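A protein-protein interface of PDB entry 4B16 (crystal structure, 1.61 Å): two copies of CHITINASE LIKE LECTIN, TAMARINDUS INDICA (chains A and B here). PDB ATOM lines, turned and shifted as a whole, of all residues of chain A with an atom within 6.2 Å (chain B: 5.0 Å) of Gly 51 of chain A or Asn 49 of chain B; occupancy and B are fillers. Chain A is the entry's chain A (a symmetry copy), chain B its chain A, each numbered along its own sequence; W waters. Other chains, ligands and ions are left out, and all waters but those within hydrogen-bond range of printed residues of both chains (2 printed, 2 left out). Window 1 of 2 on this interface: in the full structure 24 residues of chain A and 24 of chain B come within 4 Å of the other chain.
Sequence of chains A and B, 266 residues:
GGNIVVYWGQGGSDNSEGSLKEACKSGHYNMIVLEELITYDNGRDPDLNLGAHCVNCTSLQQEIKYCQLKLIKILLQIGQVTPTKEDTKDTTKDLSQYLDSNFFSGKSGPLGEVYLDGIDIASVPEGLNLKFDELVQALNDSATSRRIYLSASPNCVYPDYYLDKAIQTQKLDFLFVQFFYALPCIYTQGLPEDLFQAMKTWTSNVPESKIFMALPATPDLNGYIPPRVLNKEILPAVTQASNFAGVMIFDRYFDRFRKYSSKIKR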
ATOM      1  N   GLY A   9     -14.178   8.854  29.023  1.00  0.00           N
ATOM      2  CA  GLY A   9     -15.602   8.798  28.676  1.00  0.00           C
ATOM      3  C   GLY A   9     -16.277  10.151  28.669  1.00  0.00           C
ATOM      4  O   GLY A   9     -17.255  10.348  27.949  1.00  0.00           O
ATOM      5  N   GLN A  10     -15.754  11.085  29.465  1.00  0.00           N
ATOM      6  CA  GLN A  10     -16.331  12.429  29.557  1.00  0.00           C
ATOM      7  C   GLN A  10     -15.476  13.505  28.890  1.00  0.00           C
ATOM      8  O   GLN A  10     -15.707  14.707  29.081  1.00  0.00           O
ATOM      9  CB  GLN A  10     -16.628  12.800  31.018  1.00  0.00           C
ATOM     10  CG  GLN A  10     -17.807  12.032  31.593  1.00  0.00           C
ATOM     11  CD  GLN A  10     -19.087  12.327  30.849  1.00  0.00           C
ATOM     12  OE1 GLN A  10     -19.500  13.484  30.729  1.00  0.00           O
ATOM     13  NE2 GLN A  10     -19.724  11.284  30.339  1.00  0.00           N
ATOM     14  N   GLY A  11     -14.501  13.080  28.097  1.00  0.00           N
ATOM     15  CA  GLY A  11     -13.586  14.028  27.438  1.00  0.00           C
ATOM     16  C   GLY A  11     -14.040  14.454  26.059  1.00  0.00           C
ATOM     17  O   GLY A  11     -13.263  15.057  25.310  1.00  0.00           O
ATOM     18  N   GLY A  12     -15.288  14.122  25.714  1.00  0.00           N
ATOM     19  CA  GLY A  12     -15.935  14.612  24.500  1.00  0.00           C
ATOM     20  C   GLY A  12     -16.305  13.505  23.538  1.00  0.00           C
ATOM     21  O   GLY A  12     -17.160  12.665  23.841  1.00  0.00           O
ATOM     22  N   SER A  13     -15.658  13.502  22.374  1.00  0.00           N
ATOM     23  CA  SER A  13     -15.876  12.470  21.341  1.00  0.00           C
ATOM     24  C   SER A  13     -14.598  11.669  21.124  1.00  0.00           C
ATOM     25  O   SER A  13     -13.575  11.941  21.754  1.00  0.00           O
ATOM     26  CB  SER A  13     -16.254  13.133  20.022  1.00  0.00           C
ATOM     27  OG  SER A  13     -15.149  13.904  19.575  1.00  0.00           O
ATOM     28  N   GLU A  35     -16.484   6.837  32.490  1.00  0.00           N
ATOM     29  CA  GLU A  35     -17.377   7.838  33.063  1.00  0.00           C
ATOM     30  C   GLU A  35     -18.437   8.182  32.005  1.00  0.00           C
ATOM     31  O   GLU A  35     -18.077   8.715  30.958  1.00  0.00           O
ATOM     32  CB  GLU A  35     -16.592   9.093  33.438  1.00  0.00           C
ATOM     33  CG  GLU A  35     -15.479   8.880  34.468  1.00  0.00           C
ATOM     34  CD  GLU A  35     -14.904  10.204  34.937  1.00  0.00           C
ATOM     35  OE1 GLU A  35     -14.233  10.875  34.117  1.00  0.00           O
ATOM     36  OE2 GLU A  35     -15.123  10.575  36.123  1.00  0.00           O
ATOM     37  N   ASN A  49     -23.860   7.309  29.946  1.00  0.00           N
ATOM     38  CA  ASN A  49     -23.504   8.610  29.389  1.00  0.00           C
ATOM     39  C   ASN A  49     -22.009   8.667  29.091  1.00  0.00           C
ATOM     40  O   ASN A  49     -21.211   9.001  29.968  1.00  0.00           O
ATOM     41  CB  ASN A  49     -23.915   9.736  30.352  1.00  0.00           C
ATOM     42  CG  ASN A  49     -23.523  11.123  29.852  1.00  0.00           C
ATOM     43  OD1 ASN A  49     -22.993  11.284  28.747  1.00  0.00           O
ATOM     44  ND2 ASN A  49     -23.772  12.135  30.677  1.00  0.00           N
ATOM     45  N   LEU A  50     -21.638   8.365  27.847  1.00  0.00           N
ATOM     46  CA  LEU A  50     -20.246   8.523  27.409  1.00  0.00           C
ATOM     47  C   LEU A  50     -20.109   9.750  26.502  1.00  0.00           C
ATOM     48  O   LEU A  50     -19.338   9.761  25.539  1.00  0.00           O
ATOM     49  CB  LEU A  50     -19.740   7.244  26.728  1.00  0.00           C
ATOM     50  CG  LEU A  50     -19.722   6.011  27.651  1.00  0.00           C
ATOM     51  CD1 LEU A  50     -19.381   4.761  26.856  1.00  0.00           C
ATOM     52  CD2 LEU A  50     -18.731   6.162  28.801  1.00  0.00           C
ATOM     53  N   GLY A  51     -20.871  10.789  26.827  1.00  0.00           N
ATOM     54  CA  GLY A  51     -20.851  12.039  26.066  1.00  0.00           C
ATOM     55  C   GLY A  51     -21.026  11.836  24.575  1.00  0.00           C
ATOM     56  O   GLY A  51     -21.919  11.106  24.130  1.00  0.00           O
ATOM     57  N   ALA A  52     -20.150  12.471  23.801  1.00  0.00           N
ATOM     58  CA  ALA A  52     -20.213  12.405  22.346  1.00  0.00           C
ATOM     59  C   ALA A  52     -19.461  11.215  21.740  1.00  0.00           C
ATOM     60  O   ALA A  52     -19.282  11.152  20.520  1.00  0.00           O
ATOM     61  CB  ALA A  52     -19.736  13.719  21.741  1.00  0.00           C
ATOM     62  N   HIS A  53     -19.033  10.263  22.573  1.00  0.00           N
ATOM     63  CA  HIS A  53     -18.408   9.050  22.040  1.00  0.00           C
ATOM     64  C   HIS A  53     -19.385   8.177  21.269  1.00  0.00           C
ATOM     65  O   HIS A  53     -19.041   7.654  20.207  1.00  0.00           O
ATOM     66  CB  HIS A  53     -17.767   8.215  23.156  1.00  0.00           C
ATOM     67  CG  HIS A  53     -16.497   8.801  23.679  1.00  0.00           C
ATOM     68  ND1 HIS A  53     -15.327   8.806  22.948  1.00  0.00           N
ATOM     69  CD2 HIS A  53     -16.214   9.401  24.859  1.00  0.00           C
ATOM     70  CE1 HIS A  53     -14.376   9.386  23.660  1.00  0.00           C
ATOM     71  NE2 HIS A  53     -14.889   9.757  24.823  1.00  0.00           N
ATOM     72  N   CYS A  54     -20.598   8.033  21.812  1.00  0.00           N
ATOM     73  CA  CYS A  54     -21.620   7.130  21.266  1.00  0.00           C
ATOM     74  C   CYS A  54     -22.935   7.325  22.011  1.00  0.00           C
ATOM     75  O   CYS A  54     -22.951   7.748  23.180  1.00  0.00           O
ATOM     76  CB  CYS A  54     -21.172   5.659  21.384  1.00  0.00           C
ATOM     77  SG  CYS A  54     -20.564   5.180  23.025  1.00  0.00           S
ATOM     78  N   VAL A  55     -24.034   7.041  21.321  1.00  0.00           N
ATOM     79  CA  VAL A  55     -25.343   6.885  21.956  1.00  0.00           C
ATOM     80  C   VAL A  55     -25.670   5.389  22.041  1.00  0.00           C
ATOM     81  O   VAL A  55     -26.011   4.882  23.113  1.00  0.00           O
ATOM     82  CB  VAL A  55     -26.449   7.682  21.226  1.00  0.00           C
ATOM     83  CG1 VAL A  55     -26.464   7.368  19.737  1.00  0.00           C
ATOM     84  CG2 VAL A  55     -27.806   7.425  21.855  1.00  0.00           C
ATOM     85  N   GLY B   9     -27.934  20.686  29.024  1.00  0.00           N
ATOM     86  CA  GLY B   9     -27.258  19.874  28.007  1.00  0.00           C
ATOM     87  C   GLY B   9     -26.270  18.883  28.583  1.00  0.00           C
ATOM     88  O   GLY B   9     -26.019  17.842  27.978  1.00  0.00           O
ATOM     89  N   GLN B  10     -25.716  19.202  29.753  1.00  0.00           N
ATOM     90  CA  GLN B  10     -24.733  18.330  30.402  1.00  0.00           C
ATOM     91  C   GLN B  10     -25.275  17.617  31.640  1.00  0.00           C
ATOM     92  O   GLN B  10     -24.510  17.036  32.422  1.00  0.00           O
ATOM     93  CB  GLN B  10     -23.450  19.105  30.740  1.00  0.00           C
ATOM     94  CG  GLN B  10     -22.632  19.454  29.508  1.00  0.00           C
ATOM     95  CD  GLN B  10     -22.159  18.220  28.777  1.00  0.00           C
ATOM     96  OE1 GLN B  10     -21.495  17.355  29.356  1.00  0.00           O
ATOM     97  NE2 GLN B  10     -22.501  18.125  27.502  1.00  0.00           N
ATOM     98  N   GLU B  35     -25.038  23.389  26.633  1.00  0.00           N
ATOM     99  CA  GLU B  35     -23.682  22.927  26.905  1.00  0.00           C
ATOM    100  C   GLU B  35     -23.534  21.522  26.299  1.00  0.00           C
ATOM    101  O   GLU B  35     -24.222  20.609  26.749  1.00  0.00           O
ATOM    102  CB  GLU B  35     -23.436  22.871  28.412  1.00  0.00           C
ATOM    103  CG  GLU B  35     -23.582  24.206  29.145  1.00  0.00           C
ATOM    104  CD  GLU B  35     -23.112  24.098  30.583  1.00  0.00           C
ATOM    105  OE1 GLU B  35     -23.799  23.409  31.375  1.00  0.00           O
ATOM    106  OE2 GLU B  35     -22.056  24.699  30.924  1.00  0.00           O
ATOM    107  N   GLU B  36     -22.643  21.303  25.324  1.00  0.00           N
ATOM    108  CA  GLU B  36     -21.683  22.301  24.842  1.00  0.00           C
ATOM    109  C   GLU B  36     -21.132  21.877  23.485  1.00  0.00           C
ATOM    110  O   GLU B  36     -21.279  20.709  23.074  1.00  0.00           O
ATOM    111  CB  GLU B  36     -20.518  22.445  25.827  1.00  0.00           C
ATOM    112  CG  GLU B  36     -19.658  21.196  25.927  1.00  0.00           C
ATOM    113  CD  GLU B  36     -19.212  20.927  27.341  1.00  0.00           C
ATOM    114  OE1 GLU B  36     -19.871  21.441  28.270  1.00  0.00           O
ATOM    115  OE2 GLU B  36     -18.221  20.196  27.516  1.00  0.00           O
ATOM    116  N   LEU B  37     -20.499  22.823  22.797  1.00  0.00           N
ATOM    117  CA  LEU B  37     -19.819  22.544  21.538  1.00  0.00           C
ATOM    118  C   LEU B  37     -18.319  22.377  21.785  1.00  0.00           C
ATOM    119  O   LEU B  37     -17.698  23.212  22.444  1.00  0.00           O
ATOM    120  CB  LEU B  37     -20.052  23.702  20.548  1.00  0.00           C
ATOM    121  CG  LEU B  37     -19.589  23.443  19.105  1.00  0.00           C
ATOM    122  CD1 LEU B  37     -20.504  22.419  18.416  1.00  0.00           C
ATOM    123  CD2 LEU B  37     -19.559  24.749  18.324  1.00  0.00           C
ATOM    124  N   ILE B  38     -17.757  21.298  21.247  1.00  0.00           N
ATOM    125  CA  ILE B  38     -16.314  21.047  21.258  1.00  0.00           C
ATOM    126  C   ILE B  38     -15.741  21.596  19.957  1.00  0.00           C
ATOM    127  O   ILE B  38     -16.240  21.272  18.870  1.00  0.00           O
ATOM    128  CB  ILE B  38     -16.002  19.528  21.319  1.00  0.00           C
ATOM    129  CG1 ILE B  38     -16.675  18.857  22.529  1.00  0.00           C
ATOM    130  CG2 ILE B  38     -14.492  19.301  21.331  1.00  0.00           C
ATOM    131  CD1 ILE B  38     -16.746  17.341  22.409  1.00  0.00           C
ATOM    132  N   ASP B  47     -17.531  19.326  17.223  1.00  0.00           N
ATOM    133  CA  ASP B  47     -18.425  18.224  17.627  1.00  0.00           C
ATOM    134  C   ASP B  47     -19.392  18.718  18.693  1.00  0.00           C
ATOM    135  O   ASP B  47     -18.962  19.181  19.754  1.00  0.00           O
ATOM    136  CB  ASP B  47     -17.636  17.062  18.236  1.00  0.00           C
ATOM    137  CG  ASP B  47     -16.850  16.251  17.216  1.00  0.00           C
ATOM    138  OD1 ASP B  47     -17.300  16.087  16.057  1.00  0.00           O
ATOM    139  OD2 ASP B  47     -15.773  15.741  17.604  1.00  0.00           O
ATOM    140  N   LEU B  48     -20.688  18.566  18.447  1.00  0.00           N
ATOM    141  CA  LEU B  48     -21.689  18.876  19.463  1.00  0.00           C
ATOM    142  C   LEU B  48     -21.656  17.803  20.548  1.00  0.00           C
ATOM    143  O   LEU B  48     -21.576  16.606  20.243  1.00  0.00           O
ATOM    144  CB  LEU B  48     -23.076  18.938  18.818  1.00  0.00           C
ATOM    145  CG  LEU B  48     -24.235  19.384  19.708  1.00  0.00           C
ATOM    146  CD1 LEU B  48     -24.051  20.811  20.226  1.00  0.00           C
ATOM    147  CD2 LEU B  48     -25.528  19.246  18.914  1.00  0.00           C
ATOM    148  N   ASN B  49     -21.700  18.223  21.809  1.00  0.00           N
ATOM    149  CA  ASN B  49     -21.756  17.270  22.913  1.00  0.00           C
ATOM    150  C   ASN B  49     -22.893  17.630  23.865  1.00  0.00           C
ATOM    151  O   ASN B  49     -22.710  18.437  24.778  1.00  0.00           O
ATOM    152  CB  ASN B  49     -20.411  17.232  23.656  1.00  0.00           C
ATOM    153  CG  ASN B  49     -20.418  16.291  24.857  1.00  0.00           C
ATOM    154  OD1 ASN B  49     -21.405  15.599  25.128  1.00  0.00           O
ATOM    155  ND2 ASN B  49     -19.313  16.275  25.595  1.00  0.00           N
ATOM    156  N   LEU B  50     -24.056  17.012  23.664  1.00  0.00           N
ATOM    157  CA  LEU B  50     -25.175  17.171  24.601  1.00  0.00           C
ATOM    158  C   LEU B  50     -25.344  15.907  25.448  1.00  0.00           C
ATOM    159  O   LEU B  50     -26.458  15.497  25.786  1.00  0.00           O
ATOM    160  CB  LEU B  50     -26.464  17.540  23.853  1.00  0.00           C
ATOM    161  CG  LEU B  50     -26.387  18.883  23.103  1.00  0.00           C
ATOM    162  CD1 LEU B  50     -27.630  19.084  22.251  1.00  0.00           C
ATOM    163  CD2 LEU B  50     -26.228  20.069  24.051  1.00  0.00           C
ATOM    164  N   GLY B  51     -24.216  15.293  25.791  1.00  0.00           N
ATOM    165  CA  GLY B  51     -24.207  14.077  26.607  1.00  0.00           C
ATOM    166  C   GLY B  51     -25.134  12.999  26.086  1.00  0.00           C
ATOM    167  O   GLY B  51     -25.140  12.684  24.890  1.00  0.00           O
HETATM  168  O   HOH W   1     -19.139  14.855  28.020  1.00  0.00           O
HETATM  169  O   HOH W   2     -22.908  14.762  30.145  1.00  0.00           O
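The backbone NH (N) of His 53 of chain A is in hydrogen-bond range of the backbone carbonyl oxygen (O) of Gly 12 of chain A. The side-chain amide oxygen of Asn 49 of chain A sits at hydrogen-bond distance from the backbone NH of Gly 51 of chain A (2.9 Å). The backbone carbonyl oxygen of Glu 36 of chain B sits at hydrogen-bond distance from the backbone NH of Asn 49 of chain B (2.8 Å). The side-chain amide nitrogen of Gln 10 of chain B lies within hydrogen-bond range of the backbone carbonyl oxygen of Asn 49 of chain B. The backbone carbonyl oxygen (O) of Asn 49 of chain A lies within hydrogen-bond range of the side-chain amide nitrogen (NE2) of Gln 10 of chain A (2.7 Å). The backbone carbonyl oxygen (O) of Asp 47 of chain B sits at hydrogen-bond distance from the backbone NH (N) of Ile 38 of chain B (2.9 Å).
Asn 49 of chain A touches Gly 51 of chain B, and with the chains exchanged Gly 51 of chain A touches Asn 49 of chain B. Gly 51 of chain B touches its own counterpart, Gly 51 of chain A. 6 positions are printed for both chains. Of the 9 pairs that touch across the chains among the printed residues, 3 have their exchanged pair printed and touching as well.
CA of Gly 12 of chain A touches CD1 of Ile 38 of chain B, at 3.5 Å. Asn 49 of chain B touches Gly 12 of chain A. Ser 13 of chain A touches Ile 38 of chain B (N to CD1, 3.99 Å). CA of Gly 51 of chain B touches OD1 of Asn 49 of chain A, 3.7 Å away. CA of Gly 51 of chain A touches OD1 of Asn 49 of chain B, at 3.7 Å. Gly 51 of chain A touches Gly 51 of chain B. Ala 52 of chain A touches Leu 48 of chain B. N of Ala 52 of chain A touches OD1 of Asn 49 of chain B (3.6 Å).
Hydrophobic or aromatic side chains of chain B within 4 Å of the printed part of chain A: Ile 38. Hydrophobic or aromatic side chains of chain A within 4 Å of the printed part of chain B: Ala 52. Among the printed residues, 9 pairs touch across the chains.
Water W1 lies within hydrogen-bond range of the side-chain amide nitrogen (ND2) of Asn 49 of chain B and the side-chain amide oxygen (OE1) of Gln 10 of chain A. Water W2 bridges ND2 of Asn 49 of chain A (2.8 Å) and OE1 of Gln 10 of chain B (3.1 Å).
OG of Ser 13 of chain A is in hydrogen-bond range of OD2 of Asp 47 of chain B.
Of chain A, only Gly 12 (3.9 Å), Gly 51 (3.7 Å) and Ala 52 (3.6 Å) come within 4 Å of Asn 49 of chain B. Printed residues of chain B within 4 Å of Gly 12 of chain A: Ile 38 (3.5 Å) and Asn 49 (3.9 Å). Of the printed residues of chain B, Ser 13 of chain A touches Ile 38 and Asp 47. The nearest residue of chain A that does not touch Asn 49 of chain B is Gln 10 of chain A (5.3 Å). The nearest printed residue of chain A that does not touch Ile 38 of chain B is Ala 52 of chain A (4.7 Å).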
